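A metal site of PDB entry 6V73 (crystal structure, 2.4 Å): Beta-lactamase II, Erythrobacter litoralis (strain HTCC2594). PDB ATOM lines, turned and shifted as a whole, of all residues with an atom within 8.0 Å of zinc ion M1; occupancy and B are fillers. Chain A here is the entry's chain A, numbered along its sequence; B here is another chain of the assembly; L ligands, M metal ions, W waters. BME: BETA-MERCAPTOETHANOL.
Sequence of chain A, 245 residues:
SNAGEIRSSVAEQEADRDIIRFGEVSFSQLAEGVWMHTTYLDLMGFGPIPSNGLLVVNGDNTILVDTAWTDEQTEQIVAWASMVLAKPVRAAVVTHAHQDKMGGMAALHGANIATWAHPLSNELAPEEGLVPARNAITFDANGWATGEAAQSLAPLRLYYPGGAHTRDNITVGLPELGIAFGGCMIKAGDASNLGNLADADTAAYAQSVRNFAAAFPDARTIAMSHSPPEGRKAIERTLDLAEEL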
ATOM      1  N   ILE A  49      -8.282   3.114  -5.327  1.00  0.00           N
ATOM      2  CA  ILE A  49      -8.012   4.495  -4.927  1.00  0.00           C
ATOM      3  C   ILE A  49      -9.122   4.936  -3.984  1.00  0.00           C
ATOM      4  O   ILE A  49     -10.307   4.817  -4.340  1.00  0.00           O
ATOM      5  CB  ILE A  49      -7.948   5.433  -6.150  1.00  0.00           C
ATOM      6  CG1 ILE A  49      -6.738   5.129  -7.026  1.00  0.00           C
ATOM      7  CG2 ILE A  49      -7.860   6.892  -5.691  1.00  0.00           C
ATOM      8  CD1 ILE A  49      -6.804   5.845  -8.381  1.00  0.00           C
ATOM      9  N   PRO A  50      -8.800   5.471  -2.815  1.00  0.00           N
ATOM     10  CA  PRO A  50      -9.841   6.039  -1.949  1.00  0.00           C
ATOM     11  C   PRO A  50     -10.276   7.417  -2.401  1.00  0.00           C
ATOM     12  O   PRO A  50      -9.483   8.209  -2.912  1.00  0.00           O
ATOM     13  CB  PRO A  50      -9.139   6.116  -0.586  1.00  0.00           C
ATOM     14  CG  PRO A  50      -7.661   6.374  -0.947  1.00  0.00           C
ATOM     15  CD  PRO A  50      -7.434   5.605  -2.255  1.00  0.00           C
ATOM     16  N   SER A  51     -11.579   7.708  -2.188  1.00  0.00           N
ATOM     17  CA  SER A  51     -12.130   9.045  -2.398  1.00  0.00           C
ATOM     18  C   SER A  51     -13.033   9.425  -1.230  1.00  0.00           C
ATOM     19  O   SER A  51     -13.853   8.624  -0.792  1.00  0.00           O
ATOM     20  CB  SER A  51     -12.939   9.156  -3.675  1.00  0.00           C
ATOM     21  OG  SER A  51     -13.094  10.514  -4.008  1.00  0.00           O
ATOM     22  N   ASN A  52     -12.890  10.676  -0.764  1.00  0.00           N
ATOM     23  CA  ASN A  52     -13.524  11.167   0.457  1.00  0.00           C
ATOM     24  C   ASN A  52     -14.565  12.238   0.144  1.00  0.00           C
ATOM     25  O   ASN A  52     -14.275  13.197  -0.579  1.00  0.00           O
ATOM     26  CB  ASN A  52     -12.518  11.762   1.433  1.00  0.00           C
ATOM     27  CG  ASN A  52     -11.547  10.755   1.988  1.00  0.00           C
ATOM     28  OD1 ASN A  52     -10.472  11.120   2.449  1.00  0.00           O
ATOM     29  ND2 ASN A  52     -11.919   9.483   1.945  1.00  0.00           N
ATOM     30  N   TRP A  69     -17.574   6.756  -6.105  1.00  0.00           N
ATOM     31  CA  TRP A  69     -17.077   6.527  -7.467  1.00  0.00           C
ATOM     32  C   TRP A  69     -18.180   6.084  -8.419  1.00  0.00           C
ATOM     33  O   TRP A  69     -18.127   6.404  -9.612  1.00  0.00           O
ATOM     34  CB  TRP A  69     -15.961   5.490  -7.471  1.00  0.00           C
ATOM     35  CG  TRP A  69     -14.647   5.890  -6.829  1.00  0.00           C
ATOM     36  CD1 TRP A  69     -14.273   5.689  -5.534  1.00  0.00           C
ATOM     37  CD2 TRP A  69     -13.526   6.497  -7.489  1.00  0.00           C
ATOM     38  NE1 TRP A  69     -12.992   6.169  -5.328  1.00  0.00           N
ATOM     39  CE2 TRP A  69     -12.508   6.663  -6.509  1.00  0.00           C
ATOM     40  CE3 TRP A  69     -13.281   6.928  -8.798  1.00  0.00           C
ATOM     41  CZ2 TRP A  69     -11.262   7.258  -6.805  1.00  0.00           C
ATOM     42  CZ3 TRP A  69     -12.029   7.524  -9.087  1.00  0.00           C
ATOM     43  CH2 TRP A  69     -11.038   7.666  -8.101  1.00  0.00           C
ATOM     44  N   THR A  95     -17.631  18.699  -6.169  1.00  0.00           N
ATOM     45  CA  THR A  95     -16.532  19.654  -6.138  1.00  0.00           C
ATOM     46  C   THR A  95     -15.781  19.786  -7.462  1.00  0.00           C
ATOM     47  O   THR A  95     -14.975  20.721  -7.586  1.00  0.00           O
ATOM     48  CB  THR A  95     -15.548  19.315  -5.011  1.00  0.00           C
ATOM     49  OG1 THR A  95     -15.310  17.908  -4.952  1.00  0.00           O
ATOM     50  CG2 THR A  95     -16.159  19.736  -3.691  1.00  0.00           C
ATOM     51  N   HIS A  96     -16.011  18.896  -8.449  1.00  0.00           N
ATOM     52  CA  HIS A  96     -15.633  19.095  -9.847  1.00  0.00           C
ATOM     53  C   HIS A  96     -15.997  17.872 -10.694  1.00  0.00           C
ATOM     54  O   HIS A  96     -16.457  16.856 -10.162  1.00  0.00           O
ATOM     55  CB  HIS A  96     -14.138  19.408 -10.030  1.00  0.00           C
ATOM     56  CG  HIS A  96     -13.232  18.320  -9.549  1.00  0.00           C
ATOM     57  ND1 HIS A  96     -12.926  18.146  -8.216  1.00  0.00           N
ATOM     58  CD2 HIS A  96     -12.561  17.351 -10.211  1.00  0.00           C
ATOM     59  CE1 HIS A  96     -12.113  17.118  -8.085  1.00  0.00           C
ATOM     60  NE2 HIS A  96     -11.866  16.620  -9.286  1.00  0.00           N
ATOM     61  N   HIS A  98     -14.991  15.094 -12.100  1.00  0.00           N
ATOM     62  CA  HIS A  98     -14.227  13.859 -12.210  1.00  0.00           C
ATOM     63  C   HIS A  98     -15.028  12.742 -11.549  1.00  0.00           C
ATOM     64  O   HIS A  98     -15.914  12.992 -10.730  1.00  0.00           O
ATOM     65  CB  HIS A  98     -12.819  13.944 -11.549  1.00  0.00           C
ATOM     66  CG  HIS A  98     -11.775  14.578 -12.416  1.00  0.00           C
ATOM     67  ND1 HIS A  98     -10.565  15.003 -11.908  1.00  0.00           N
ATOM     68  CD2 HIS A  98     -11.752  14.857 -13.745  1.00  0.00           C
ATOM     69  CE1 HIS A  98      -9.844  15.531 -12.891  1.00  0.00           C
ATOM     70  NE2 HIS A  98     -10.551  15.457 -14.009  1.00  0.00           N
ATOM     71  N   GLN A  99     -14.672  11.511 -11.890  1.00  0.00           N
ATOM     72  CA  GLN A  99     -15.512  10.381 -11.514  1.00  0.00           C
ATOM     73  C   GLN A  99     -15.548  10.148 -10.017  1.00  0.00           C
ATOM     74  O   GLN A  99     -16.582   9.701  -9.493  1.00  0.00           O
ATOM     75  CB  GLN A  99     -15.065   9.114 -12.232  1.00  0.00           C
ATOM     76  CG  GLN A  99     -16.120   8.033 -12.130  1.00  0.00           C
ATOM     77  CD  GLN A  99     -15.589   6.693 -12.530  1.00  0.00           C
ATOM     78  OE1 GLN A  99     -14.706   6.588 -13.383  1.00  0.00           O
ATOM     79  NE2 GLN A  99     -16.111   5.654 -11.894  1.00  0.00           N
ATOM     80  N   ASP A 100     -14.457  10.415  -9.293  1.00  0.00           N
ATOM     81  CA  ASP A 100     -14.536  10.202  -7.844  1.00  0.00           C
ATOM     82  C   ASP A 100     -15.479  11.194  -7.161  1.00  0.00           C
ATOM     83  O   ASP A 100     -15.939  10.918  -6.060  1.00  0.00           O
ATOM     84  CB  ASP A 100     -13.146  10.269  -7.204  1.00  0.00           C
ATOM     85  CG  ASP A 100     -12.341  11.448  -7.658  1.00  0.00           C
ATOM     86  OD1 ASP A 100     -11.468  11.887  -6.888  1.00  0.00           O
ATOM     87  OD2 ASP A 100     -12.571  11.939  -8.792  1.00  0.00           O
ATOM     88  N   LYS A 101     -15.767  12.347  -7.794  1.00  0.00           N
ATOM     89  CA  LYS A 101     -16.648  13.344  -7.181  1.00  0.00           C
ATOM     90  C   LYS A 101     -18.059  13.355  -7.772  1.00  0.00           C
ATOM     91  O   LYS A 101     -18.994  13.749  -7.054  1.00  0.00           O
ATOM     92  CB  LYS A 101     -16.026  14.755  -7.281  1.00  0.00           C
ATOM     93  CG  LYS A 101     -14.635  14.900  -6.601  1.00  0.00           C
ATOM     94  CD  LYS A 101     -14.522  13.933  -5.415  1.00  0.00           C
ATOM     95  CE  LYS A 101     -13.969  14.541  -4.170  1.00  0.00           C
ATOM     96  NZ  LYS A 101     -13.740  13.508  -3.141  1.00  0.00           N
ATOM     97  N   HIS A 165      -6.458  21.934  -9.243  1.00  0.00           N
ATOM     98  CA  HIS A 165      -6.543  20.532  -9.659  1.00  0.00           C
ATOM     99  C   HIS A 165      -7.353  20.383 -10.947  1.00  0.00           C
ATOM    100  O   HIS A 165      -6.978  19.595 -11.824  1.00  0.00           O
ATOM    101  CB  HIS A 165      -7.146  19.692  -8.532  1.00  0.00           C
ATOM    102  CG  HIS A 165      -7.565  18.319  -8.965  1.00  0.00           C
ATOM    103  ND1 HIS A 165      -6.661  17.309  -9.239  1.00  0.00           N
ATOM    104  CD2 HIS A 165      -8.799  17.788  -9.180  1.00  0.00           C
ATOM    105  CE1 HIS A 165      -7.316  16.224  -9.590  1.00  0.00           C
ATOM    106  NE2 HIS A 165      -8.616  16.484  -9.568  1.00  0.00           N
ATOM    107  N   THR A 166      -8.467  21.112 -11.064  1.00  0.00           N
ATOM    108  CA  THR A 166      -9.149  21.337 -12.328  1.00  0.00           C
ATOM    109  C   THR A 166      -9.596  22.789 -12.381  1.00  0.00           C
ATOM    110  O   THR A 166      -9.494  23.526 -11.395  1.00  0.00           O
ATOM    111  CB  THR A 166     -10.370  20.421 -12.522  1.00  0.00           C
ATOM    112  OG1 THR A 166     -11.334  20.747 -11.529  1.00  0.00           O
ATOM    113  CG2 THR A 166     -10.027  18.945 -12.411  1.00  0.00           C
ATOM    114  N   GLY A 183     -11.298  19.340  -1.296  1.00  0.00           N
ATOM    115  CA  GLY A 183     -11.459  18.466  -2.438  1.00  0.00           C
ATOM    116  C   GLY A 183     -10.143  17.835  -2.852  1.00  0.00           C
ATOM    117  O   GLY A 183      -9.314  17.454  -2.011  1.00  0.00           O
ATOM    118  N   CYS A 184      -9.967  17.705  -4.157  1.00  0.00           N
ATOM    119  CA  CYS A 184      -8.760  17.163  -4.761  1.00  0.00           C
ATOM    120  C   CYS A 184      -7.672  18.205  -4.964  1.00  0.00           C
ATOM    121  O   CYS A 184      -6.548  17.833  -5.308  1.00  0.00           O
ATOM    122  CB  CYS A 184      -9.072  16.507  -6.091  1.00  0.00           C
ATOM    123  SG  CYS A 184     -10.320  15.209  -6.009  1.00  0.00           S
ATOM    124  N   MET A 185      -7.994  19.492  -4.765  1.00  0.00           N
ATOM    125  CA  MET A 185      -6.965  20.520  -4.871  1.00  0.00           C
ATOM    126  C   MET A 185      -5.923  20.368  -3.779  1.00  0.00           C
ATOM    127  O   MET A 185      -4.727  20.567  -4.013  1.00  0.00           O
ATOM    128  CB  MET A 185      -7.601  21.898  -4.802  1.00  0.00           C
ATOM    129  CG  MET A 185      -6.595  23.017  -4.634  1.00  0.00           C
ATOM    130  SD  MET A 185      -7.326  24.654  -4.691  1.00  0.00           S
ATOM    131  CE  MET A 185      -8.170  24.712  -3.116  1.00  0.00           C
ATOM    132  N   ILE A 186      -6.360  20.027  -2.567  1.00  0.00           N
ATOM    133  CA  ILE A 186      -5.490  19.933  -1.406  1.00  0.00           C
ATOM    134  C   ILE A 186      -4.999  18.504  -1.288  1.00  0.00           C
ATOM    135  O   ILE A 186      -5.787  17.560  -1.392  1.00  0.00           O
ATOM    136  CB  ILE A 186      -6.218  20.372  -0.128  1.00  0.00           C
ATOM    137  CG1 ILE A 186      -6.601  21.846  -0.196  1.00  0.00           C
ATOM    138  CG2 ILE A 186      -5.360  20.081   1.095  1.00  0.00           C
ATOM    139  CD1 ILE A 186      -5.411  22.814  -0.162  1.00  0.00           C
ATOM    140  N   LYS A 187      -3.686  18.351  -1.080  1.00  0.00           N
ATOM    141  CA  LYS A 187      -3.085  17.045  -0.873  1.00  0.00           C
ATOM    142  C   LYS A 187      -2.404  17.025   0.493  1.00  0.00           C
ATOM    143  O   LYS A 187      -2.293  18.058   1.167  1.00  0.00           O
ATOM    144  CB  LYS A 187      -2.117  16.705  -2.002  1.00  0.00           C
ATOM    145  CG  LYS A 187      -2.672  15.690  -3.007  1.00  0.00           C
ATOM    146  CD  LYS A 187      -3.610  16.316  -4.029  1.00  0.00           C
ATOM    147  CE  LYS A 187      -4.328  15.216  -4.790  1.00  0.00           C
ATOM    148  NZ  LYS A 187      -4.730  15.631  -6.153  1.00  0.00           N
ATOM    149  N   LEU A 194       1.140  16.295  -6.605  1.00  0.00           N
ATOM    150  CA  LEU A 194      -0.243  16.739  -6.536  1.00  0.00           C
ATOM    151  C   LEU A 194      -1.209  15.756  -7.173  1.00  0.00           C
ATOM    152  O   LEU A 194      -2.288  16.154  -7.594  1.00  0.00           O
ATOM    153  CB  LEU A 194      -0.357  18.114  -7.191  1.00  0.00           C
ATOM    154  CG  LEU A 194       0.395  19.151  -6.377  1.00  0.00           C
ATOM    155  CD1 LEU A 194       0.595  20.438  -7.158  1.00  0.00           C
ATOM    156  CD2 LEU A 194      -0.367  19.414  -5.078  1.00  0.00           C
ATOM    157  N   GLY A 195      -0.832  14.482  -7.255  1.00  0.00           N
ATOM    158  CA  GLY A 195      -1.767  13.499  -7.791  1.00  0.00           C
ATOM    159  C   GLY A 195      -2.001  13.704  -9.272  1.00  0.00           C
ATOM    160  O   GLY A 195      -1.069  13.897 -10.043  1.00  0.00           O
ATOM    161  N   ASN A 196      -3.265  13.669  -9.682  1.00  0.00           N
ATOM    162  CA  ASN A 196      -3.609  13.623 -11.100  1.00  0.00           C
ATOM    163  C   ASN A 196      -3.770  15.038 -11.637  1.00  0.00           C
ATOM    164  O   ASN A 196      -4.780  15.703 -11.386  1.00  0.00           O
ATOM    165  CB  ASN A 196      -4.873  12.799 -11.314  1.00  0.00           C
ATOM    166  CG  ASN A 196      -5.455  12.995 -12.697  1.00  0.00           C
ATOM    167  OD1 ASN A 196      -4.724  13.145 -13.687  1.00  0.00           O
ATOM    168  ND2 ASN A 196      -6.779  12.996 -12.780  1.00  0.00           N
ATOM    169  N   MET A 224      -9.747  16.360   2.742  1.00  0.00           N
ATOM    170  CA  MET A 224      -9.460  16.340   1.302  1.00  0.00           C
ATOM    171  C   MET A 224      -9.876  15.005   0.722  1.00  0.00           C
ATOM    172  O   MET A 224     -10.242  14.066   1.447  1.00  0.00           O
ATOM    173  CB  MET A 224      -7.976  16.612   1.036  1.00  0.00           C
ATOM    174  CG  MET A 224      -7.079  15.465   1.421  1.00  0.00           C
ATOM    175  SD  MET A 224      -5.457  16.020   1.957  1.00  0.00           S
ATOM    176  CE  MET A 224      -5.768  16.506   3.653  1.00  0.00           C
ATOM    177  N   SER A 225      -9.794  14.908  -0.610  1.00  0.00           N
ATOM    178  CA  SER A 225     -10.405  13.778  -1.313  1.00  0.00           C
ATOM    179  C   SER A 225      -9.643  12.472  -1.117  1.00  0.00           C
ATOM    180  O   SER A 225     -10.264  11.398  -1.102  1.00  0.00           O
ATOM    181  CB  SER A 225     -10.502  14.072  -2.801  1.00  0.00           C
ATOM    182  OG  SER A 225     -11.331  15.197  -3.044  1.00  0.00           O
ATOM    183  N   HIS A 226      -8.313  12.507  -1.006  1.00  0.00           N
ATOM    184  CA  HIS A 226      -7.567  11.267  -1.200  1.00  0.00           C
ATOM    185  C   HIS A 226      -6.648  10.904  -0.040  1.00  0.00           C
ATOM    186  O   HIS A 226      -5.842   9.977  -0.183  1.00  0.00           O
ATOM    187  CB  HIS A 226      -6.775  11.322  -2.519  1.00  0.00           C
ATOM    188  CG  HIS A 226      -7.659  11.409  -3.723  1.00  0.00           C
ATOM    189  ND1 HIS A 226      -8.534  10.411  -4.081  1.00  0.00           N
ATOM    190  CD2 HIS A 226      -7.832  12.396  -4.637  1.00  0.00           C
ATOM    191  CE1 HIS A 226      -9.196  10.767  -5.174  1.00  0.00           C
ATOM    192  NE2 HIS A 226      -8.783  11.967  -5.535  1.00  0.00           N
ATOM    193  N   PHE B  46      -0.926   7.387  -5.116  1.00  0.00           N
ATOM    194  CA  PHE B  46      -1.870   6.313  -4.881  1.00  0.00           C
ATOM    195  C   PHE B  46      -1.181   4.965  -4.714  1.00  0.00           C
ATOM    196  O   PHE B  46      -1.843   3.931  -4.708  1.00  0.00           O
ATOM    197  CB  PHE B  46      -2.884   6.225  -6.019  1.00  0.00           C
ATOM    198  CG  PHE B  46      -3.600   7.524  -6.294  1.00  0.00           C
ATOM    199  CD1 PHE B  46      -4.040   8.314  -5.270  1.00  0.00           C
ATOM    200  CD2 PHE B  46      -3.848   7.930  -7.599  1.00  0.00           C
ATOM    201  CE1 PHE B  46      -4.711   9.497  -5.521  1.00  0.00           C
ATOM    202  CE2 PHE B  46      -4.532   9.117  -7.851  1.00  0.00           C
ATOM    203  CZ  PHE B  46      -4.954   9.897  -6.814  1.00  0.00           C
HETATM  204  C1  BME L   1      -8.889  11.590 -10.790  1.00  0.00           C
HETATM  205  C2  BME L   1      -8.505  12.760  -9.877  1.00  0.00           C
HETATM  206  O1  BME L   1      -8.354  10.380 -10.278  1.00  0.00           O
HETATM  207  S2  BME L   1      -9.970  13.390  -8.967  1.00  0.00           S
HETATM  208 ZN    ZN M   1      -9.467  13.331  -6.990  1.00  0.00          ZN
HETATM  209 ZN    ZN M   2     -10.301  15.262  -9.838  1.00  0.00          ZN
HETATM  210  O   HOH W   1      -6.236  13.526  -7.861  1.00  0.00           O
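The backbone NH of Cys 184 sits at hydrogen-bond distance from the side-chain hydroxyl of Ser 225 (3.1 Å). The backbone carbonyl oxygen (O) of Cys 184 is in hydrogen-bond range of the side-chain amino group (NZ) of Lys 187, 3.0 Å away. The backbone carbonyl oxygen of Pro 50 is in hydrogen-bond range of a ring nitrogen (ND1) of His 226 (2.7 Å).
Within 4 Å of zinc ion M1: Asp 100, Cys 184 and His 226. The nearest printed residue that does not touch zinc ion M1 is His 165 (4.2 Å).
Zinc ion M1 is bound by S2 of the ligand (2.0 Å), NE2 of His 226 (2.1 Å), SG of Cys 184 (2.3 Å) and OD1 of Asp 100 (2.5 Å).
Water W1 lies within hydrogen-bond range of the side-chain amino group of Lys 187 (3.1 Å) and the backbone NH of Asn 196 (3.5 Å).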
